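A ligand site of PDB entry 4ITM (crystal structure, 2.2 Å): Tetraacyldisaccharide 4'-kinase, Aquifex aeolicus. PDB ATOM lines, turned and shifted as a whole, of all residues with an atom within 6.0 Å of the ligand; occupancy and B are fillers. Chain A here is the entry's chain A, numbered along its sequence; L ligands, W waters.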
ATOM      1  N   GLY A  47     -17.280 -39.269  21.955  1.00  0.00           N
ATOM      2  CA  GLY A  47     -18.336 -38.267  21.928  1.00  0.00           C
ATOM      3  C   GLY A  47     -17.752 -36.864  21.853  1.00  0.00           C
ATOM      4  O   GLY A  47     -16.543 -36.674  22.049  1.00  0.00           O
ATOM      5  N   GLY A  48     -18.601 -35.875  21.582  1.00  0.00           N
ATOM      6  CA  GLY A  48     -18.130 -34.502  21.433  1.00  0.00           C
ATOM      7  C   GLY A  48     -17.580 -33.914  22.724  1.00  0.00           C
ATOM      8  O   GLY A  48     -18.075 -34.199  23.803  1.00  0.00           O
ATOM      9  N   SER A  49     -16.546 -33.091  22.609  1.00  0.00           N
ATOM     10  CA  SER A  49     -16.035 -32.381  23.781  1.00  0.00           C
ATOM     11  C   SER A  49     -15.756 -30.934  23.443  1.00  0.00           C
ATOM     12  O   SER A  49     -14.819 -30.329  23.991  1.00  0.00           O
ATOM     13  CB  SER A  49     -14.778 -33.063  24.330  1.00  0.00           C
ATOM     14  OG  SER A  49     -15.068 -34.362  24.820  1.00  0.00           O
ATOM     15  N   GLY A  50     -16.549 -30.369  22.528  1.00  0.00           N
ATOM     16  CA  GLY A  50     -16.451 -28.959  22.189  1.00  0.00           C
ATOM     17  C   GLY A  50     -15.352 -28.579  21.208  1.00  0.00           C
ATOM     18  O   GLY A  50     -14.910 -27.421  21.157  1.00  0.00           O
ATOM     19  N   LYS A  51     -14.918 -29.539  20.401  1.00  0.00           N
ATOM     20  CA  LYS A  51     -13.779 -29.287  19.509  1.00  0.00           C
ATOM     21  C   LYS A  51     -13.987 -28.214  18.427  1.00  0.00           C
ATOM     22  O   LYS A  51     -13.097 -27.428  18.157  1.00  0.00           O
ATOM     23  CB  LYS A  51     -13.257 -30.588  18.898  1.00  0.00           C
ATOM     24  CG  LYS A  51     -12.961 -30.546  17.413  1.00  0.00           C
ATOM     25  CD  LYS A  51     -13.548 -31.802  16.790  1.00  0.00           C
ATOM     26  CE  LYS A  51     -13.257 -31.898  15.315  1.00  0.00           C
ATOM     27  NZ  LYS A  51     -14.049 -30.931  14.506  1.00  0.00           N
ATOM     28  N   THR A  52     -15.156 -28.193  17.806  1.00  0.00           N
ATOM     29  CA  THR A  52     -15.398 -27.187  16.770  1.00  0.00           C
ATOM     30  C   THR A  52     -15.317 -25.797  17.387  1.00  0.00           C
ATOM     31  O   THR A  52     -14.635 -24.941  16.848  1.00  0.00           O
ATOM     32  CB  THR A  52     -16.755 -27.403  16.100  1.00  0.00           C
ATOM     33  OG1 THR A  52     -16.814 -28.756  15.607  1.00  0.00           O
ATOM     34  CG2 THR A  52     -16.980 -26.381  14.958  1.00  0.00           C
ATOM     35  N   SER A  53     -15.967 -25.593  18.525  1.00  0.00           N
ATOM     36  CA  SER A  53     -15.861 -24.329  19.251  1.00  0.00           C
ATOM     37  C   SER A  53     -14.399 -23.961  19.519  1.00  0.00           C
ATOM     38  O   SER A  53     -13.975 -22.842  19.232  1.00  0.00           O
ATOM     39  CB  SER A  53     -16.610 -24.380  20.578  1.00  0.00           C
ATOM     40  OG  SER A  53     -18.006 -24.252  20.376  1.00  0.00           O
ATOM     41  N   MET A  56     -12.559 -22.907  16.524  1.00  0.00           N
ATOM     42  CA  MET A  56     -12.962 -21.540  16.167  1.00  0.00           C
ATOM     43  C   MET A  56     -12.198 -20.522  17.004  1.00  0.00           C
ATOM     44  O   MET A  56     -11.651 -19.542  16.480  1.00  0.00           O
ATOM     45  CB  MET A  56     -14.488 -21.358  16.322  1.00  0.00           C
ATOM     46  CG  MET A  56     -15.311 -22.160  15.305  1.00  0.00           C
ATOM     47  SD  MET A  56     -17.051 -22.326  15.753  1.00  0.00           S
ATOM     48  CE  MET A  56     -17.659 -20.636  15.522  1.00  0.00           C
ATOM     49  N   GLU A 100     -17.975 -32.898   8.289  1.00  0.00           N
ATOM     50  CA  GLU A 100     -17.213 -32.177   9.303  1.00  0.00           C
ATOM     51  C   GLU A 100     -16.112 -31.253   8.777  1.00  0.00           C
ATOM     52  O   GLU A 100     -15.970 -30.126   9.257  1.00  0.00           O
ATOM     53  CB  GLU A 100     -16.649 -33.146  10.330  1.00  0.00           C
ATOM     54  CG  GLU A 100     -16.028 -32.460  11.496  1.00  0.00           C
ATOM     55  CD  GLU A 100     -16.400 -33.135  12.792  1.00  0.00           C
ATOM     56  OE1 GLU A 100     -17.180 -34.108  12.743  1.00  0.00           O
ATOM     57  OE2 GLU A 100     -15.912 -32.693  13.849  1.00  0.00           O
ATOM     58  N   LEU A 103     -17.889 -28.325   7.189  1.00  0.00           N
ATOM     59  CA  LEU A 103     -18.513 -27.403   8.129  1.00  0.00           C
ATOM     60  C   LEU A 103     -17.466 -26.491   8.752  1.00  0.00           C
ATOM     61  O   LEU A 103     -17.699 -25.290   8.911  1.00  0.00           O
ATOM     62  CB  LEU A 103     -19.318 -28.157   9.199  1.00  0.00           C
ATOM     63  CG  LEU A 103     -19.782 -27.321  10.392  1.00  0.00           C
ATOM     64  CD1 LEU A 103     -20.658 -26.136   9.966  1.00  0.00           C
ATOM     65  CD2 LEU A 103     -20.516 -28.216  11.380  1.00  0.00           C
ATOM     66  N   LEU A 107     -17.368 -22.525   8.941  1.00  0.00           N
ATOM     67  CA  LEU A 107     -17.304 -21.798  10.205  1.00  0.00           C
ATOM     68  C   LEU A 107     -16.058 -20.904  10.298  1.00  0.00           C
ATOM     69  O   LEU A 107     -16.026 -19.969  11.097  1.00  0.00           O
ATOM     70  CB  LEU A 107     -17.390 -22.770  11.379  1.00  0.00           C
ATOM     71  CG  LEU A 107     -18.811 -23.306  11.557  1.00  0.00           C
ATOM     72  CD1 LEU A 107     -18.891 -24.337  12.663  1.00  0.00           C
ATOM     73  CD2 LEU A 107     -19.762 -22.139  11.831  1.00  0.00           C
ATOM     74  N   TYR A 187     -17.802 -28.247  28.143  1.00  0.00           N
ATOM     75  CA  TYR A 187     -19.163 -28.481  28.603  1.00  0.00           C
ATOM     76  C   TYR A 187     -19.449 -27.793  29.949  1.00  0.00           C
ATOM     77  O   TYR A 187     -20.204 -28.304  30.772  1.00  0.00           O
ATOM     78  CB  TYR A 187     -19.474 -29.983  28.636  1.00  0.00           C
ATOM     79  CG  TYR A 187     -19.772 -30.557  27.268  1.00  0.00           C
ATOM     80  CD1 TYR A 187     -18.836 -30.499  26.236  1.00  0.00           C
ATOM     81  CD2 TYR A 187     -21.001 -31.152  26.997  1.00  0.00           C
ATOM     82  CE1 TYR A 187     -19.117 -31.013  24.968  1.00  0.00           C
ATOM     83  CE2 TYR A 187     -21.294 -31.679  25.743  1.00  0.00           C
ATOM     84  CZ  TYR A 187     -20.352 -31.607  24.738  1.00  0.00           C
ATOM     85  OH  TYR A 187     -20.665 -32.139  23.505  1.00  0.00           O
ATOM     86  N   MET A 204     -13.528 -23.372  29.026  1.00  0.00           N
ATOM     87  CA  MET A 204     -14.127 -22.833  27.818  1.00  0.00           C
ATOM     88  C   MET A 204     -15.622 -22.533  28.029  1.00  0.00           C
ATOM     89  O   MET A 204     -16.343 -23.341  28.640  1.00  0.00           O
ATOM     90  CB  MET A 204     -13.964 -23.836  26.664  1.00  0.00           C
ATOM     91  CG  MET A 204     -14.559 -23.364  25.347  1.00  0.00           C
ATOM     92  SD  MET A 204     -14.204 -24.421  23.937  1.00  0.00           S
ATOM     93  CE  MET A 204     -15.539 -25.597  24.070  1.00  0.00           C
ATOM     94  N   ARG A 206     -19.237 -20.860  25.919  1.00  0.00           N
ATOM     95  CA  ARG A 206     -19.881 -20.363  24.710  1.00  0.00           C
ATOM     96  C   ARG A 206     -20.965 -19.377  25.096  1.00  0.00           C
ATOM     97  O   ARG A 206     -21.625 -19.541  26.119  1.00  0.00           O
ATOM     98  CB  ARG A 206     -20.488 -21.504  23.888  1.00  0.00           C
ATOM     99  CG  ARG A 206     -19.535 -22.147  22.875  1.00  0.00           C
ATOM    100  CD  ARG A 206     -18.431 -22.949  23.564  1.00  0.00           C
ATOM    101  NE  ARG A 206     -18.979 -24.014  24.404  1.00  0.00           N
ATOM    102  CZ  ARG A 206     -19.400 -25.185  23.946  1.00  0.00           C
ATOM    103  NH1 ARG A 206     -19.338 -25.474  22.647  1.00  0.00           N
ATOM    104  NH2 ARG A 206     -19.882 -26.079  24.799  1.00  0.00           N
ATOM    105  N   LEU A 212     -26.397 -17.513  11.862  1.00  0.00           N
ATOM    106  CA  LEU A 212     -25.667 -17.701  10.619  1.00  0.00           C
ATOM    107  C   LEU A 212     -26.677 -17.908   9.494  1.00  0.00           C
ATOM    108  O   LEU A 212     -27.584 -18.712   9.624  1.00  0.00           O
ATOM    109  CB  LEU A 212     -24.728 -18.901  10.741  1.00  0.00           C
ATOM    110  CG  LEU A 212     -23.574 -18.751  11.723  1.00  0.00           C
ATOM    111  CD1 LEU A 212     -22.974 -20.106  12.025  1.00  0.00           C
ATOM    112  CD2 LEU A 212     -22.501 -17.770  11.175  1.00  0.00           C
ATOM    113  N   GLN A 240     -30.594 -31.550  22.238  1.00  0.00           N
ATOM    114  CA  GLN A 240     -29.786 -30.366  22.568  1.00  0.00           C
ATOM    115  C   GLN A 240     -30.373 -29.096  21.937  1.00  0.00           C
ATOM    116  O   GLN A 240     -30.568 -28.083  22.619  1.00  0.00           O
ATOM    117  CB  GLN A 240     -28.332 -30.572  22.112  1.00  0.00           C
ATOM    118  CG  GLN A 240     -27.362 -29.476  22.521  1.00  0.00           C
ATOM    119  CD  GLN A 240     -25.909 -29.825  22.178  1.00  0.00           C
ATOM    120  OE1 GLN A 240     -25.618 -30.931  21.721  1.00  0.00           O
ATOM    121  NE2 GLN A 240     -24.992 -28.883  22.406  1.00  0.00           N
ATOM    122  N   PRO A 279     -25.808 -25.991  12.457  1.00  0.00           N
ATOM    123  CA  PRO A 279     -24.825 -25.731  11.391  1.00  0.00           C
ATOM    124  C   PRO A 279     -24.522 -26.983  10.556  1.00  0.00           C
ATOM    125  O   PRO A 279     -24.277 -26.848   9.358  1.00  0.00           O
ATOM    126  CB  PRO A 279     -23.603 -25.236  12.175  1.00  0.00           C
ATOM    127  CG  PRO A 279     -24.219 -24.563  13.373  1.00  0.00           C
ATOM    128  CD  PRO A 279     -25.363 -25.473  13.754  1.00  0.00           C
ATOM    129  N   LYS A 280     -24.594 -28.171  11.164  1.00  0.00           N
ATOM    130  CA  LYS A 280     -24.367 -29.415  10.440  1.00  0.00           C
ATOM    131  C   LYS A 280     -25.453 -29.670   9.408  1.00  0.00           C
ATOM    132  O   LYS A 280     -25.213 -30.316   8.381  1.00  0.00           O
ATOM    133  CB  LYS A 280     -24.256 -30.610  11.386  1.00  0.00           C
ATOM    134  CG  LYS A 280     -22.857 -30.862  11.922  1.00  0.00           C
ATOM    135  CD  LYS A 280     -22.739 -32.160  12.726  1.00  0.00           C
ATOM    136  CE  LYS A 280     -23.665 -32.183  13.945  1.00  0.00           C
ATOM    137  NZ  LYS A 280     -23.422 -33.371  14.817  1.00  0.00           N
ATOM    138  N   LEU A 294     -27.710 -20.972  14.693  1.00  0.00           N
ATOM    139  CA  LEU A 294     -27.265 -20.130  15.806  1.00  0.00           C
ATOM    140  C   LEU A 294     -25.746 -20.092  15.797  1.00  0.00           C
ATOM    141  O   LEU A 294     -25.096 -21.098  15.562  1.00  0.00           O
ATOM    142  CB  LEU A 294     -27.741 -20.699  17.141  1.00  0.00           C
ATOM    143  CG  LEU A 294     -29.222 -21.011  17.342  1.00  0.00           C
ATOM    144  CD1 LEU A 294     -29.441 -21.711  18.673  1.00  0.00           C
ATOM    145  CD2 LEU A 294     -30.053 -19.759  17.270  1.00  0.00           C
ATOM    146  N   ASN A 295     -25.197 -18.909  16.068  1.00  0.00           N
ATOM    147  CA  ASN A 295     -23.762 -18.730  16.152  1.00  0.00           C
ATOM    148  C   ASN A 295     -23.398 -18.340  17.579  1.00  0.00           C
ATOM    149  O   ASN A 295     -24.040 -17.480  18.174  1.00  0.00           O
ATOM    150  CB  ASN A 295     -23.329 -17.632  15.162  1.00  0.00           C
ATOM    151  CG  ASN A 295     -21.833 -17.389  15.171  1.00  0.00           C
ATOM    152  OD1 ASN A 295     -21.033 -18.313  15.029  1.00  0.00           O
ATOM    153  ND2 ASN A 295     -21.450 -16.143  15.357  1.00  0.00           N
ATOM    154  N   PHE A 296     -22.372 -18.988  18.143  1.00  0.00           N
ATOM    155  CA  PHE A 296     -21.947 -18.712  19.513  1.00  0.00           C
ATOM    156  C   PHE A 296     -20.507 -18.222  19.550  1.00  0.00           C
ATOM    157  O   PHE A 296     -19.629 -18.790  18.889  1.00  0.00           O
ATOM    158  CB  PHE A 296     -22.058 -19.979  20.384  1.00  0.00           C
ATOM    159  CG  PHE A 296     -23.467 -20.420  20.623  1.00  0.00           C
ATOM    160  CD1 PHE A 296     -24.114 -21.239  19.700  1.00  0.00           C
ATOM    161  CD2 PHE A 296     -24.152 -20.031  21.760  1.00  0.00           C
ATOM    162  CE1 PHE A 296     -25.406 -21.649  19.911  1.00  0.00           C
ATOM    163  CE2 PHE A 296     -25.457 -20.443  21.972  1.00  0.00           C
ATOM    164  CZ  PHE A 296     -26.085 -21.252  21.047  1.00  0.00           C
ATOM    165  N   LYS A 297     -20.268 -17.170  20.332  1.00  0.00           N
ATOM    166  CA  LYS A 297     -18.908 -16.718  20.613  1.00  0.00           C
ATOM    167  C   LYS A 297     -18.263 -17.738  21.527  1.00  0.00           C
ATOM    168  O   LYS A 297     -18.936 -18.334  22.378  1.00  0.00           O
ATOM    169  CB  LYS A 297     -18.908 -15.348  21.317  1.00  0.00           C
ATOM    170  CG  LYS A 297     -19.412 -14.177  20.482  1.00  0.00           C
ATOM    171  CD  LYS A 297     -19.387 -12.871  21.282  1.00  0.00           C
ATOM    172  CE  LYS A 297     -19.962 -11.681  20.505  1.00  0.00           C
ATOM    173  NZ  LYS A 297     -19.182 -11.372  19.276  1.00  0.00           N
ATOM    174  N   VAL A 298     -16.968 -17.960  21.351  1.00  0.00           N
ATOM    175  CA  VAL A 298     -16.234 -18.915  22.178  1.00  0.00           C
ATOM    176  C   VAL A 298     -15.194 -18.184  23.015  1.00  0.00           C
ATOM    177  O   VAL A 298     -14.389 -17.416  22.473  1.00  0.00           O
ATOM    178  CB  VAL A 298     -15.548 -19.970  21.329  1.00  0.00           C
ATOM    179  CG1 VAL A 298     -14.870 -21.035  22.221  1.00  0.00           C
ATOM    180  CG2 VAL A 298     -16.566 -20.611  20.391  1.00  0.00           C
HETATM  181  P1  LIG L   1     -18.104 -31.163  18.034  1.00  0.00           P
HETATM  182  O1  LIG L   1     -17.427 -32.352  18.657  1.00  0.00           O
HETATM  183  O2  LIG L   1     -17.201 -30.024  17.636  1.00  0.00           O
HETATM  184  O3  LIG L   1     -19.123 -31.516  16.982  1.00  0.00           O
HETATM  185  P2  LIG L   1     -19.869 -31.280  20.303  1.00  0.00           P
HETATM  186  O4  LIG L   1     -19.125 -31.446  21.603  1.00  0.00           O
HETATM  187  O5  LIG L   1     -20.482 -32.504  19.673  1.00  0.00           O
HETATM  188  O6  LIG L   1     -18.998 -30.494  19.204  1.00  0.00           O
HETATM  189  P3  LIG L   1     -21.018 -28.677  20.921  1.00  0.00           P
HETATM  190  O7  LIG L   1     -22.068 -28.656  22.009  1.00  0.00           O
HETATM  191  O8  LIG L   1     -19.662 -28.123  21.231  1.00  0.00           O
HETATM  192  O9  LIG L   1     -21.066 -30.231  20.503  1.00  0.00           O
HETATM  193  O10 LIG L   1     -21.610 -27.916  19.623  1.00  0.00           O
HETATM  194  C1  LIG L   1     -22.659 -28.546  18.857  1.00  0.00           C
HETATM  195  C2  LIG L   1     -22.490 -28.329  17.345  1.00  0.00           C
HETATM  196  O11 LIG L   1     -22.668 -26.949  16.984  1.00  0.00           O
HETATM  197  C3  LIG L   1     -21.114 -28.730  16.839  1.00  0.00           C
HETATM  198  O12 LIG L   1     -21.094 -30.115  16.486  1.00  0.00           O
HETATM  199  C4  LIG L   1     -20.863 -27.771  15.676  1.00  0.00           C
HETATM  200  O13 LIG L   1     -21.491 -28.226  14.470  1.00  0.00           O
HETATM  201  C5  LIG L   1     -21.663 -26.532  16.057  1.00  0.00           C
HETATM  202  N1  LIG L   1     -20.859 -25.519  16.782  1.00  0.00           N
HETATM  203  C6  LIG L   1     -19.829 -25.759  17.615  1.00  0.00           C
HETATM  204  N2  LIG L   1     -19.354 -24.604  18.138  1.00  0.00           N
HETATM  205  C7  LIG L   1     -20.106 -23.604  17.629  1.00  0.00           C
HETATM  206  C8  LIG L   1     -20.142 -22.135  17.769  1.00  0.00           C
HETATM  207  N3  LIG L   1     -19.257 -21.494  18.576  1.00  0.00           N
HETATM  208  N4  LIG L   1     -21.089 -21.465  17.057  1.00  0.00           N
HETATM  209  C9  LIG L   1     -21.982 -22.097  16.259  1.00  0.00           C
HETATM  210  N5  LIG L   1     -22.005 -23.433  16.090  1.00  0.00           N
HETATM  211  C10 LIG L   1     -21.104 -24.211  16.734  1.00  0.00           C
HETATM  212  O   HOH W   1     -24.287 -28.609  14.041  1.00  0.00           O
HETATM  213  O   HOH W   2     -15.400 -32.663  20.143  1.00  0.00           O
HETATM  214  O   HOH W   3     -21.566 -28.666  24.535  1.00  0.00           O
HETATM  215  O   HOH W   4     -17.832 -27.506  19.456  1.00  0.00           O
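N of Thr 52 lies within hydrogen-bond range of O2 of the ligand (2.8 Å). OG1 of Thr 52 lies within hydrogen-bond range of O2 of the ligand (2.4 Å). The side-chain hydroxyl of Tyr 187 sits at hydrogen-bond distance from an oxygen (O4) of the ligand. OG of Ser 53 sits at hydrogen-bond distance from N2 of the ligand, 2.6 Å away. N4 of the ligand lies within hydrogen-bond range of N of Phe 296 (3.0 Å). A nitrogen (N3) of the ligand sits at hydrogen-bond distance from the backbone carbonyl oxygen (O) of Phe 296, at 2.7 Å. N of Gly 50 lies within hydrogen-bond range of O4 of the ligand (2.9 Å). The side-chain amide nitrogen (NE2) of Gln 240 sits at hydrogen-bond distance from an oxygen (O7) of the ligand (3.0 Å). An oxygen (O8) of the ligand lies within salt-bridge range of the guanidinium group (NH1) of Arg 206, at 3.0 Å. O4 of the ligand is in hydrogen-bond range of N of Ser 49 (3.2 Å). The side-chain sulfur of Met 56 sits close to a nitrogen (N3) of the ligand, 3.7 Å away.
The side-chain hydroxyl (OH) of Tyr 187 is in hydrogen-bond range of the backbone carbonyl oxygen (O) of Gly 48. The guanidinium group (NH1) of Arg 206 is in hydrogen-bond range of the side-chain hydroxyl (OG) of Ser 53 (2.9 Å). The side-chain carboxylate of Glu 100 lies within salt-bridge range of the side-chain amino group of Lys 51 (2.6 Å).
C of Gly 48 touches O4 of the ligand, at 3.1 Å. Lys 51 touches the ligand. CD2 of Leu 103 touches O13 of the ligand, at 3.2 Å. CG of Pro 279 touches N5 of the ligand, at 3.7 Å. Lys 280 touches the ligand. Leu 294 touches the ligand. Asn 295 touches the ligand. Val 298 touches the ligand (CG2 to N3, 3.4 Å). The nearest printed residue that does not touch the ligand is Leu 107 (4.6 Å).
Water W2 lies within hydrogen-bond range of O1 of the ligand, N of Ser 49 and N of Lys 51. Water W3 bridges O7 of the ligand and NH2 of Arg 206. Water W4 lies within hydrogen-bond range of an oxygen (O8) of the ligand (2.6 Å), the backbone NH of Ser 53 (2.8 Å), the backbone NH of Thr 52 (3.2 Å) and the backbone carbonyl oxygen of Gly 50 (3.4 Å). Water W1 bridges an oxygen (O13) of the ligand (2.9 Å) and the backbone NH (N) of Lys 280 (2.9 Å).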
